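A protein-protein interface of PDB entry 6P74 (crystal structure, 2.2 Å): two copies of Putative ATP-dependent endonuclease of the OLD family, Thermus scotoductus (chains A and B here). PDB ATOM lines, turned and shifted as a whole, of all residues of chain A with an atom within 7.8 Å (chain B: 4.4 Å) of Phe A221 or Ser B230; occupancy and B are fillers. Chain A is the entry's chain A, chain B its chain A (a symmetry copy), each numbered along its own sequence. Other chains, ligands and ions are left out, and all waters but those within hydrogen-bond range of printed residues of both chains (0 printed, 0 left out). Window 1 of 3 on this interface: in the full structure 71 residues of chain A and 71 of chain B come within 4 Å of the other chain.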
ATOM      1  N   SER A 150     -12.642  19.584 -30.614  1.00  0.00           N
ATOM      2  CA  SER A 150     -11.573  19.165 -29.714  1.00  0.00           C
ATOM      3  C   SER A 150     -10.364  18.734 -30.536  1.00  0.00           C
ATOM      4  O   SER A 150     -10.475  18.425 -31.724  1.00  0.00           O
ATOM      5  CB  SER A 150     -12.015  18.020 -28.801  1.00  0.00           C
ATOM      6  OG  SER A 150     -11.815  16.774 -29.443  1.00  0.00           O
ATOM      7  N   PHE A 173      -7.861  11.605  -7.751  1.00  0.00           N
ATOM      8  CA  PHE A 173      -8.509  11.720  -9.051  1.00  0.00           C
ATOM      9  C   PHE A 173      -9.327  10.478  -9.382  1.00  0.00           C
ATOM     10  O   PHE A 173     -10.406  10.578  -9.980  1.00  0.00           O
ATOM     11  CB  PHE A 173      -7.480  11.972 -10.147  1.00  0.00           C
ATOM     12  CG  PHE A 173      -8.100  12.134 -11.488  1.00  0.00           C
ATOM     13  CD1 PHE A 173      -8.542  13.379 -11.911  1.00  0.00           C
ATOM     14  CD2 PHE A 173      -8.305  11.033 -12.309  1.00  0.00           C
ATOM     15  CE1 PHE A 173      -9.143  13.529 -13.138  1.00  0.00           C
ATOM     16  CE2 PHE A 173      -8.901  11.182 -13.538  1.00  0.00           C
ATOM     17  CZ  PHE A 173      -9.324  12.432 -13.956  1.00  0.00           C
ATOM     18  N   VAL A 176     -12.813  10.706  -7.605  1.00  0.00           N
ATOM     19  CA  VAL A 176     -13.721  11.684  -8.193  1.00  0.00           C
ATOM     20  C   VAL A 176     -14.106  11.263  -9.604  1.00  0.00           C
ATOM     21  O   VAL A 176     -15.266  11.395 -10.014  1.00  0.00           O
ATOM     22  CB  VAL A 176     -13.106  13.091  -8.165  1.00  0.00           C
ATOM     23  CG1 VAL A 176     -14.099  14.095  -8.727  1.00  0.00           C
ATOM     24  CG2 VAL A 176     -12.715  13.465  -6.740  1.00  0.00           C
ATOM     25  N   TYR A 177     -13.150  10.726 -10.362  1.00  0.00           N
ATOM     26  CA  TYR A 177     -13.451  10.266 -11.714  1.00  0.00           C
ATOM     27  C   TYR A 177     -14.532   9.180 -11.705  1.00  0.00           C
ATOM     28  O   TYR A 177     -15.533   9.280 -12.429  1.00  0.00           O
ATOM     29  CB  TYR A 177     -12.173   9.769 -12.393  1.00  0.00           C
ATOM     30  CG  TYR A 177     -12.452   9.078 -13.702  1.00  0.00           C
ATOM     31  CD1 TYR A 177     -12.647   9.818 -14.876  1.00  0.00           C
ATOM     32  CD2 TYR A 177     -12.546   7.691 -13.769  1.00  0.00           C
ATOM     33  CE1 TYR A 177     -12.916   9.195 -16.064  1.00  0.00           C
ATOM     34  CE2 TYR A 177     -12.816   7.057 -14.963  1.00  0.00           C
ATOM     35  CZ  TYR A 177     -12.998   7.811 -16.106  1.00  0.00           C
ATOM     36  OH  TYR A 177     -13.267   7.189 -17.298  1.00  0.00           O
ATOM     37  N   GLU A 178     -14.351   8.137 -10.882  1.00  0.00           N
ATOM     38  CA  GLU A 178     -15.359   7.079 -10.781  1.00  0.00           C
ATOM     39  C   GLU A 178     -16.700   7.633 -10.324  1.00  0.00           C
ATOM     40  O   GLU A 178     -17.758   7.202 -10.799  1.00  0.00           O
ATOM     41  CB  GLU A 178     -14.895   5.989  -9.814  1.00  0.00           C
ATOM     42  CG  GLU A 178     -13.688   5.207 -10.295  1.00  0.00           C
ATOM     43  CD  GLU A 178     -13.912   4.558 -11.651  1.00  0.00           C
ATOM     44  OE1 GLU A 178     -12.923   4.403 -12.402  1.00  0.00           O
ATOM     45  OE2 GLU A 178     -15.074   4.208 -11.962  1.00  0.00           O
ATOM     46  N   ALA A 180     -17.907  10.450 -11.060  1.00  0.00           N
ATOM     47  CA  ALA A 180     -18.553  11.036 -12.228  1.00  0.00           C
ATOM     48  C   ALA A 180     -19.036   9.959 -13.189  1.00  0.00           C
ATOM     49  O   ALA A 180     -20.118  10.083 -13.773  1.00  0.00           O
ATOM     50  CB  ALA A 180     -17.598  11.999 -12.926  1.00  0.00           C
ATOM     51  N   MET A 181     -18.250   8.895 -13.373  1.00  0.00           N
ATOM     52  CA  MET A 181     -18.695   7.804 -14.236  1.00  0.00           C
ATOM     53  C   MET A 181     -19.966   7.142 -13.710  1.00  0.00           C
ATOM     54  O   MET A 181     -20.785   6.661 -14.502  1.00  0.00           O
ATOM     55  CB  MET A 181     -17.582   6.766 -14.402  1.00  0.00           C
ATOM     56  CG  MET A 181     -16.579   7.109 -15.494  1.00  0.00           C
ATOM     57  SD  MET A 181     -17.332   7.315 -17.137  1.00  0.00           S
ATOM     58  CE  MET A 181     -17.972   5.661 -17.402  1.00  0.00           C
ATOM     59  N   ASP A 182     -20.158   7.117 -12.386  1.00  0.00           N
ATOM     60  CA  ASP A 182     -21.360   6.509 -11.828  1.00  0.00           C
ATOM     61  C   ASP A 182     -22.616   7.295 -12.175  1.00  0.00           C
ATOM     62  O   ASP A 182     -23.696   6.702 -12.283  1.00  0.00           O
ATOM     63  CB  ASP A 182     -21.231   6.372 -10.312  1.00  0.00           C
ATOM     64  CG  ASP A 182     -20.248   5.290  -9.909  1.00  0.00           C
ATOM     65  OD1 ASP A 182     -19.952   4.414 -10.758  1.00  0.00           O
ATOM     66  OD2 ASP A 182     -19.773   5.321  -8.751  1.00  0.00           O
ATOM     67  N   LEU A 184     -23.155   8.539 -14.990  1.00  0.00           N
ATOM     68  CA  LEU A 184     -23.465   8.130 -16.354  1.00  0.00           C
ATOM     69  C   LEU A 184     -24.002   6.709 -16.424  1.00  0.00           C
ATOM     70  O   LEU A 184     -24.812   6.397 -17.307  1.00  0.00           O
ATOM     71  CB  LEU A 184     -22.218   8.236 -17.229  1.00  0.00           C
ATOM     72  CG  LEU A 184     -21.612   9.629 -17.305  1.00  0.00           C
ATOM     73  CD1 LEU A 184     -20.556   9.669 -18.404  1.00  0.00           C
ATOM     74  CD2 LEU A 184     -22.710  10.671 -17.526  1.00  0.00           C
ATOM     75  N   GLY A 218     -14.769  -1.445 -20.737  1.00  0.00           N
ATOM     76  CA  GLY A 218     -15.903  -0.659 -20.294  1.00  0.00           C
ATOM     77  C   GLY A 218     -15.848   0.734 -20.881  1.00  0.00           C
ATOM     78  O   GLY A 218     -14.931   1.085 -21.628  1.00  0.00           O
ATOM     79  N   PHE A 219     -16.858   1.520 -20.528  1.00  0.00           N
ATOM     80  CA  PHE A 219     -16.949   2.919 -20.910  1.00  0.00           C
ATOM     81  C   PHE A 219     -16.089   3.795 -19.993  1.00  0.00           C
ATOM     82  O   PHE A 219     -15.696   3.397 -18.892  1.00  0.00           O
ATOM     83  CB  PHE A 219     -18.402   3.387 -20.847  1.00  0.00           C
ATOM     84  CG  PHE A 219     -19.274   2.873 -21.969  1.00  0.00           C
ATOM     85  CD1 PHE A 219     -18.883   3.000 -23.293  1.00  0.00           C
ATOM     86  CD2 PHE A 219     -20.508   2.291 -21.689  1.00  0.00           C
ATOM     87  CE1 PHE A 219     -19.705   2.534 -24.328  1.00  0.00           C
ATOM     88  CE2 PHE A 219     -21.329   1.831 -22.712  1.00  0.00           C
ATOM     89  CZ  PHE A 219     -20.936   1.962 -24.030  1.00  0.00           C
ATOM     90  N   GLY A 220     -15.814   5.006 -20.457  1.00  0.00           N
ATOM     91  CA  GLY A 220     -15.063   5.978 -19.689  1.00  0.00           C
ATOM     92  C   GLY A 220     -14.509   7.049 -20.604  1.00  0.00           C
ATOM     93  O   GLY A 220     -14.637   6.977 -21.830  1.00  0.00           O
ATOM     94  N   PHE A 221     -13.884   8.064 -19.983  1.00  0.00           N
ATOM     95  CA  PHE A 221     -13.177   9.067 -20.775  1.00  0.00           C
ATOM     96  C   PHE A 221     -11.764   9.332 -20.273  1.00  0.00           C
ATOM     97  O   PHE A 221     -11.195  10.381 -20.593  1.00  0.00           O
ATOM     98  CB  PHE A 221     -13.943  10.390 -20.862  1.00  0.00           C
ATOM     99  CG  PHE A 221     -14.875  10.615 -19.750  1.00  0.00           C
ATOM    100  CD1 PHE A 221     -14.404  11.015 -18.511  1.00  0.00           C
ATOM    101  CD2 PHE A 221     -16.234  10.440 -19.936  1.00  0.00           C
ATOM    102  CE1 PHE A 221     -15.278  11.224 -17.464  1.00  0.00           C
ATOM    103  CE2 PHE A 221     -17.118  10.639 -18.899  1.00  0.00           C
ATOM    104  CZ  PHE A 221     -16.639  11.033 -17.657  1.00  0.00           C
ATOM    105  N   ALA A 222     -11.172   8.405 -19.527  1.00  0.00           N
ATOM    106  CA  ALA A 222      -9.771   8.583 -19.177  1.00  0.00           C
ATOM    107  C   ALA A 222      -9.268   7.319 -18.511  1.00  0.00           C
ATOM    108  O   ALA A 222     -10.046   6.568 -17.919  1.00  0.00           O
ATOM    109  CB  ALA A 222      -9.567   9.817 -18.286  1.00  0.00           C
ATOM    110  N   ASP A 223      -7.959   7.092 -18.618  1.00  0.00           N
ATOM    111  CA  ASP A 223      -7.307   6.129 -17.740  1.00  0.00           C
ATOM    112  C   ASP A 223      -7.082   6.854 -16.417  1.00  0.00           C
ATOM    113  O   ASP A 223      -6.249   7.769 -16.348  1.00  0.00           O
ATOM    114  CB  ASP A 223      -5.982   5.646 -18.334  1.00  0.00           C
ATOM    115  CG  ASP A 223      -5.373   4.473 -17.560  1.00  0.00           C
ATOM    116  OD1 ASP A 223      -5.441   4.456 -16.310  1.00  0.00           O
ATOM    117  OD2 ASP A 223      -4.818   3.563 -18.216  1.00  0.00           O
ATOM    118  N   PRO A 224      -7.815   6.504 -15.357  1.00  0.00           N
ATOM    119  CA  PRO A 224      -7.642   7.226 -14.083  1.00  0.00           C
ATOM    120  C   PRO A 224      -6.238   7.120 -13.520  1.00  0.00           C
ATOM    121  O   PRO A 224      -5.830   7.994 -12.745  1.00  0.00           O
ATOM    122  CB  PRO A 224      -8.680   6.577 -13.155  1.00  0.00           C
ATOM    123  CG  PRO A 224      -9.047   5.282 -13.818  1.00  0.00           C
ATOM    124  CD  PRO A 224      -8.872   5.484 -15.292  1.00  0.00           C
ATOM    125  N   PRO A 227      -4.132  10.199 -16.163  1.00  0.00           N
ATOM    126  CA  PRO A 227      -5.196  11.056 -16.720  1.00  0.00           C
ATOM    127  C   PRO A 227      -4.710  12.027 -17.786  1.00  0.00           C
ATOM    128  O   PRO A 227      -5.446  12.303 -18.745  1.00  0.00           O
ATOM    129  CB  PRO A 227      -5.728  11.790 -15.481  1.00  0.00           C
ATOM    130  CG  PRO A 227      -4.553  11.838 -14.559  1.00  0.00           C
ATOM    131  CD  PRO A 227      -3.811  10.544 -14.768  1.00  0.00           C
ATOM    132  N   ASN A 229      -3.079  11.511 -20.190  1.00  0.00           N
ATOM    133  CA  ASN A 229      -3.063  10.869 -21.501  1.00  0.00           C
ATOM    134  C   ASN A 229      -4.387  10.975 -22.241  1.00  0.00           C
ATOM    135  O   ASN A 229      -4.467  10.565 -23.401  1.00  0.00           O
ATOM    136  CB  ASN A 229      -2.686   9.391 -21.377  1.00  0.00           C
ATOM    137  CG  ASN A 229      -1.237   9.129 -21.742  1.00  0.00           C
ATOM    138  OD1 ASN A 229      -0.394  10.035 -21.703  1.00  0.00           O
ATOM    139  ND2 ASN A 229      -0.937   7.882 -22.094  1.00  0.00           N
ATOM    140  N   SER A 230      -5.422  11.497 -21.606  1.00  0.00           N
ATOM    141  CA  SER A 230      -6.701  11.732 -22.254  1.00  0.00           C
ATOM    142  C   SER A 230      -7.075  13.207 -22.265  1.00  0.00           C
ATOM    143  O   SER A 230      -8.150  13.561 -22.768  1.00  0.00           O
ATOM    144  CB  SER A 230      -7.798  10.916 -21.554  1.00  0.00           C
ATOM    145  OG  SER A 230      -7.242  10.084 -20.544  1.00  0.00           O
ATOM    146  N   LEU A 231      -6.234  14.075 -21.715  1.00  0.00           N
ATOM    147  CA  LEU A 231      -6.528  15.497 -21.728  1.00  0.00           C
ATOM    148  C   LEU A 231      -6.465  16.028 -23.159  1.00  0.00           C
ATOM    149  O   LEU A 231      -5.607  15.636 -23.952  1.00  0.00           O
ATOM    150  CB  LEU A 231      -5.546  16.242 -20.830  1.00  0.00           C
ATOM    151  CG  LEU A 231      -6.053  17.208 -19.773  1.00  0.00           C
ATOM    152  CD1 LEU A 231      -7.167  16.617 -18.906  1.00  0.00           C
ATOM    153  CD2 LEU A 231      -4.877  17.601 -18.911  1.00  0.00           C
ATOM    154  N   ARG A 232      -7.396  16.912 -23.491  1.00  0.00           N
ATOM    155  CA  ARG A 232      -7.416  17.552 -24.792  1.00  0.00           C
ATOM    156  C   ARG A 232      -7.672  19.038 -24.598  1.00  0.00           C
ATOM    157  O   ARG A 232      -8.071  19.480 -23.520  1.00  0.00           O
ATOM    158  CB  ARG A 232      -8.483  16.918 -25.686  1.00  0.00           C
ATOM    159  CG  ARG A 232      -9.684  16.426 -24.911  1.00  0.00           C
ATOM    160  CD  ARG A 232     -10.775  15.911 -25.826  1.00  0.00           C
ATOM    161  NE  ARG A 232     -12.088  15.969 -25.181  1.00  0.00           N
ATOM    162  CZ  ARG A 232     -13.225  15.614 -25.773  1.00  0.00           C
ATOM    163  NH1 ARG A 232     -13.213  15.171 -27.025  1.00  0.00           N
ATOM    164  NH2 ARG A 232     -14.374  15.699 -25.116  1.00  0.00           N
ATOM    165  N   GLN A 234     -10.199  21.952 -25.641  1.00  0.00           N
ATOM    166  CA  GLN A 234     -11.562  22.005 -26.149  1.00  0.00           C
ATOM    167  C   GLN A 234     -12.073  23.438 -26.092  1.00  0.00           C
ATOM    168  O   GLN A 234     -11.472  24.308 -25.459  1.00  0.00           O
ATOM    169  CB  GLN A 234     -12.479  21.040 -25.386  1.00  0.00           C
ATOM    170  CG  GLN A 234     -12.124  20.889 -23.932  1.00  0.00           C
ATOM    171  CD  GLN A 234     -12.795  19.692 -23.292  1.00  0.00           C
ATOM    172  OE1 GLN A 234     -12.711  18.571 -23.797  1.00  0.00           O
ATOM    173  NE2 GLN A 234     -13.467  19.925 -22.173  1.00  0.00           N
ATOM    174  N   PHE B 173     -23.491  15.835 -13.103  1.00  0.00           N
ATOM    175  CA  PHE B 173     -22.253  15.433 -13.756  1.00  0.00           C
ATOM    176  C   PHE B 173     -21.290  16.604 -13.903  1.00  0.00           C
ATOM    177  O   PHE B 173     -20.071  16.435 -13.767  1.00  0.00           O
ATOM    178  CB  PHE B 173     -22.537  14.818 -15.122  1.00  0.00           C
ATOM    179  CG  PHE B 173     -21.302  14.358 -15.809  1.00  0.00           C
ATOM    180  CD1 PHE B 173     -20.802  13.085 -15.577  1.00  0.00           C
ATOM    181  CD2 PHE B 173     -20.596  15.215 -16.643  1.00  0.00           C
ATOM    182  CE1 PHE B 173     -19.646  12.664 -16.188  1.00  0.00           C
ATOM    183  CE2 PHE B 173     -19.442  14.795 -17.260  1.00  0.00           C
ATOM    184  CZ  PHE B 173     -18.962  13.516 -17.032  1.00  0.00           C
ATOM    185  N   PHE B 221     -11.526  16.484 -20.509  1.00  0.00           N
ATOM    186  CA  PHE B 221     -11.767  15.254 -21.260  1.00  0.00           C
ATOM    187  C   PHE B 221     -13.240  15.020 -21.557  1.00  0.00           C
ATOM    188  O   PHE B 221     -13.626  13.882 -21.844  1.00  0.00           O
ATOM    189  CB  PHE B 221     -11.185  14.021 -20.563  1.00  0.00           C
ATOM    190  CG  PHE B 221     -11.029  14.174 -19.110  1.00  0.00           C
ATOM    191  CD1 PHE B 221     -12.128  14.079 -18.274  1.00  0.00           C
ATOM    192  CD2 PHE B 221      -9.779  14.402 -18.566  1.00  0.00           C
ATOM    193  CE1 PHE B 221     -11.984  14.226 -16.909  1.00  0.00           C
ATOM    194  CE2 PHE B 221      -9.620  14.555 -17.207  1.00  0.00           C
ATOM    195  CZ  PHE B 221     -10.725  14.468 -16.373  1.00  0.00           C
ATOM    196  N   ALA B 222     -14.067  16.061 -21.530  1.00  0.00           N
ATOM    197  CA  ALA B 222     -15.443  15.869 -21.966  1.00  0.00           C
ATOM    198  C   ALA B 222     -16.123  17.221 -22.043  1.00  0.00           C
ATOM    199  O   ALA B 222     -15.735  18.161 -21.347  1.00  0.00           O
ATOM    200  CB  ALA B 222     -16.196  14.903 -21.041  1.00  0.00           C
ATOM    201  N   ASP B 223     -17.140  17.306 -22.900  1.00  0.00           N
ATOM    202  CA  ASP B 223     -18.086  18.411 -22.809  1.00  0.00           C
ATOM    203  C   ASP B 223     -19.050  18.047 -21.686  1.00  0.00           C
ATOM    204  O   ASP B 223     -19.858  17.118 -21.843  1.00  0.00           O
ATOM    205  CB  ASP B 223     -18.831  18.612 -24.131  1.00  0.00           C
ATOM    206  CG  ASP B 223     -19.667  19.895 -24.155  1.00  0.00           C
ATOM    207  OD1 ASP B 223     -20.288  20.248 -23.127  1.00  0.00           O
ATOM    208  OD2 ASP B 223     -19.700  20.552 -25.220  1.00  0.00           O
ATOM    209  N   ASN B 226     -22.663  17.585 -22.769  1.00  0.00           N
ATOM    210  CA  ASN B 226     -22.966  16.404 -23.577  1.00  0.00           C
ATOM    211  C   ASN B 226     -21.879  15.362 -23.342  1.00  0.00           C
ATOM    212  O   ASN B 226     -20.997  15.162 -24.191  1.00  0.00           O
ATOM    213  CB  ASN B 226     -23.079  16.769 -25.058  1.00  0.00           C
ATOM    214  CG  ASN B 226     -23.591  15.620 -25.903  1.00  0.00           C
ATOM    215  OD1 ASN B 226     -24.222  14.690 -25.396  1.00  0.00           O
ATOM    216  ND2 ASN B 226     -23.321  15.679 -27.202  1.00  0.00           N
ATOM    217  N   PRO B 227     -21.922  14.663 -22.203  1.00  0.00           N
ATOM    218  CA  PRO B 227     -20.797  13.778 -21.841  1.00  0.00           C
ATOM    219  C   PRO B 227     -20.702  12.524 -22.698  1.00  0.00           C
ATOM    220  O   PRO B 227     -19.588  12.062 -22.989  1.00  0.00           O
ATOM    221  CB  PRO B 227     -21.086  13.442 -20.371  1.00  0.00           C
ATOM    222  CG  PRO B 227     -22.572  13.546 -20.263  1.00  0.00           C
ATOM    223  CD  PRO B 227     -22.976  14.675 -21.175  1.00  0.00           C
ATOM    224  N   PHE B 228     -21.840  11.964 -23.119  1.00  0.00           N
ATOM    225  CA  PHE B 228     -21.846  10.793 -23.984  1.00  0.00           C
ATOM    226  C   PHE B 228     -21.186  11.040 -25.347  1.00  0.00           C
ATOM    227  O   PHE B 228     -21.088  10.106 -26.148  1.00  0.00           O
ATOM    228  CB  PHE B 228     -23.286  10.303 -24.136  1.00  0.00           C
ATOM    229  CG  PHE B 228     -23.902   9.909 -22.835  1.00  0.00           C
ATOM    230  CD1 PHE B 228     -23.659   8.656 -22.290  1.00  0.00           C
ATOM    231  CD2 PHE B 228     -24.688  10.796 -22.131  1.00  0.00           C
ATOM    232  CE1 PHE B 228     -24.205   8.284 -21.073  1.00  0.00           C
ATOM    233  CE2 PHE B 228     -25.235  10.434 -20.916  1.00  0.00           C
ATOM    234  CZ  PHE B 228     -24.997   9.171 -20.385  1.00  0.00           C
ATOM    235  N   ASN B 229     -20.717  12.253 -25.636  1.00  0.00           N
ATOM    236  CA  ASN B 229     -19.967  12.521 -26.859  1.00  0.00           C
ATOM    237  C   ASN B 229     -18.466  12.330 -26.700  1.00  0.00           C
ATOM    238  O   ASN B 229     -17.736  12.423 -27.689  1.00  0.00           O
ATOM    239  CB  ASN B 229     -20.231  13.944 -27.356  1.00  0.00           C
ATOM    240  CG  ASN B 229     -21.222  13.984 -28.503  1.00  0.00           C
ATOM    241  OD1 ASN B 229     -22.020  13.056 -28.692  1.00  0.00           O
ATOM    242  ND2 ASN B 229     -21.181  15.066 -29.277  1.00  0.00           N
ATOM    243  N   SER B 230     -17.989  12.079 -25.494  1.00  0.00           N
ATOM    244  CA  SER B 230     -16.587  11.784 -25.252  1.00  0.00           C
ATOM    245  C   SER B 230     -16.385  10.394 -24.668  1.00  0.00           C
ATOM    246  O   SER B 230     -15.243  10.006 -24.391  1.00  0.00           O
ATOM    247  CB  SER B 230     -15.985  12.841 -24.314  1.00  0.00           C
ATOM    248  OG  SER B 230     -16.932  13.863 -24.032  1.00  0.00           O
ATOM    249  N   LEU B 231     -17.457   9.638 -24.458  1.00  0.00           N
ATOM    250  CA  LEU B 231     -17.319   8.290 -23.932  1.00  0.00           C
ATOM    251  C   LEU B 231     -16.636   7.396 -24.965  1.00  0.00           C
ATOM    252  O   LEU B 231     -16.890   7.495 -26.168  1.00  0.00           O
ATOM    253  CB  LEU B 231     -18.687   7.734 -23.554  1.00  0.00           C
ATOM    254  CG  LEU B 231     -18.915   7.125 -22.181  1.00  0.00           C
ATOM    255  CD1 LEU B 231     -18.408   8.012 -21.040  1.00  0.00           C
ATOM    256  CD2 LEU B 231     -20.398   6.882 -22.029  1.00  0.00           C
ATOM    257  N   ARG B 232     -15.748   6.534 -24.490  1.00  0.00           N
ATOM    258  CA  ARG B 232     -15.075   5.576 -25.347  1.00  0.00           C
ATOM    259  C   ARG B 232     -15.087   4.219 -24.660  1.00  0.00           C
ATOM    260  O   ARG B 232     -15.374   4.112 -23.467  1.00  0.00           O
ATOM    261  CB  ARG B 232     -13.647   6.034 -25.647  1.00  0.00           C
ATOM    262  CG  ARG B 232     -13.026   6.808 -24.506  1.00  0.00           C
ATOM    263  CD  ARG B 232     -11.575   7.149 -24.778  1.00  0.00           C
ATOM    264  NE  ARG B 232     -10.834   7.368 -23.536  1.00  0.00           N
ATOM    265  CZ  ARG B 232      -9.534   7.645 -23.483  1.00  0.00           C
ATOM    266  NH1 ARG B 232      -8.827   7.738 -24.604  1.00  0.00           N
ATOM    267  NH2 ARG B 232      -8.937   7.829 -22.312  1.00  0.00           N
ATOM    268  N   GLN B 234     -12.641   1.346 -23.346  1.00  0.00           N
ATOM    269  CA  GLN B 234     -11.230   1.270 -22.996  1.00  0.00           C
ATOM    270  C   GLN B 234     -10.948  -0.051 -22.293  1.00  0.00           C
ATOM    271  O   GLN B 234     -11.865  -0.768 -21.886  1.00  0.00           O
ATOM    272  CB  GLN B 234     -10.802   2.472 -22.145  1.00  0.00           C
ATOM    273  CG  GLN B 234     -11.876   2.974 -21.219  1.00  0.00           C
ATOM    274  CD  GLN B 234     -11.568   4.347 -20.661  1.00  0.00           C
ATOM    275  OE1 GLN B 234     -11.274   5.283 -21.406  1.00  0.00           O
ATOM    276  NE2 GLN B 234     -11.633   4.473 -19.343  1.00  0.00           N
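Among the printed residues, merely in contact across the chains: Phe A219 with Arg B232 (3.2 Å), Ala A222 with Arg B232 (3.3 Å), Arg A232 with Ala B222 (3.3 Å), Phe A221 with Leu B231 (3.4 Å), Leu A231 with Phe B221 (3.4 Å), Phe A173 with Phe B221 (3.5 Å), Phe A221 with Phe B173 (3.5 Å), Ala A180 with Phe B173 (3.6 Å), Gly A218 with Arg B232 (3.6 Å), Phe A221 with Phe B221 (3.6 Å), Leu A184 with Phe B173 (3.6 Å), Gly A220 with Leu B231 (3.7 Å), Gly A220 with Gln B234 (3.8 Å), Tyr A177 with Gln B234 (3.8 Å), Ser A230 with Phe B221 (3.8 Å), Phe A221 with Ser B230 (3.8 Å), Leu A184 with Leu B231 (3.8 Å), Phe A221 with Arg B232 (3.8 Å), Arg A232 with Phe B221 (3.8 Å), Arg A232 with Asp B223 (3.9 Å), Asp A223 with Arg B232 (3.9 Å), Leu A184 with Phe B228 (3.96 Å) and Leu A184 with Pro B227 (3.97 Å).
Printed residues of chain B that touch a printed residue of chain A: Phe B173, Phe B221, Ala B222, Asp B223, Pro B227, Phe B228, Ser B230, Leu B231, Arg B232 and Gln B234.
The side-chain hydroxyl of Ser A150 is in hydrogen-bond range of the guanidinium group of Arg A232, at 3.2 Å.
N of Phe A221 sits at hydrogen-bond distance from OH of Tyr A177.
The backbone NH (N) of Ala A222 is in hydrogen-bond range of the side-chain hydroxyl (OH) of Tyr A177, 3.3 Å away.
O of Pro A227 is in hydrogen-bond range of OG of Ser A230 (3.4 Å).
NE of Arg A232 is in hydrogen-bond range of OE1 of Gln A234 (3.0 Å).
OG of Ser B230 sits at hydrogen-bond distance from O of Pro B227 (3.4 Å).
Of chain B, only Phe B173 (3.5 Å), Phe B221 (3.6 Å), Ser B230 (3.8 Å), Leu B231 (3.4 Å) and Arg B232 (3.8 Å) come within 4 Å of Phe A221.
Printed residues of chain A within 4 Å of Ser B230: Phe A221 and Arg A232.
Printed residues of chain A within 4 Å of Ala B222: Arg A232 (3.3 Å) and Gln A234 (3.0 Å).
Of the printed residues of chain B, Ala A222 touches Arg B232 (3.3 Å) and Gln B234 (3.0 Å).
Of the printed residues of chain B, Leu A231 touches Phe B221 (3.4 Å).
The nearest residue of chain B that does not touch Phe A221 is Gln B234 (4.1 Å).
O of Gly A218 lies within hydrogen-bond range of N of Gln B234, 2.9 Å away.
N of Arg B232 lies within hydrogen-bond range of O of Gly A220, at 2.9 Å.
NE2 of Gln B234 is in hydrogen-bond range of O of Ala A222.
NH2 of Arg B232 sits at hydrogen-bond distance from OG of Ser A230 (3.3 Å).
The guanidinium group (NH2) of Arg A232 sits at hydrogen-bond distance from the side-chain hydroxyl (OG) of Ser B230 (3.3 Å).
NE2 of Gln A234 sits at hydrogen-bond distance from O of Ala B222 (3.0 Å).
Phe A173 touches Phe B221, and with the chains exchanged Phe A221 touches Phe B173.
Phe A221 touches Leu B231, and with the chains exchanged Leu A231 touches Phe B221.
Ala A222 touches Arg B232, and with the chains exchanged Arg A232 touches Ala B222.
Asp A223 touches Arg B232, and with the chains exchanged Arg A232 touches Asp B223.
Positions printed for both chains: 173, 221, 222, 223, 227, 229, 230, 231, 232 and 234.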
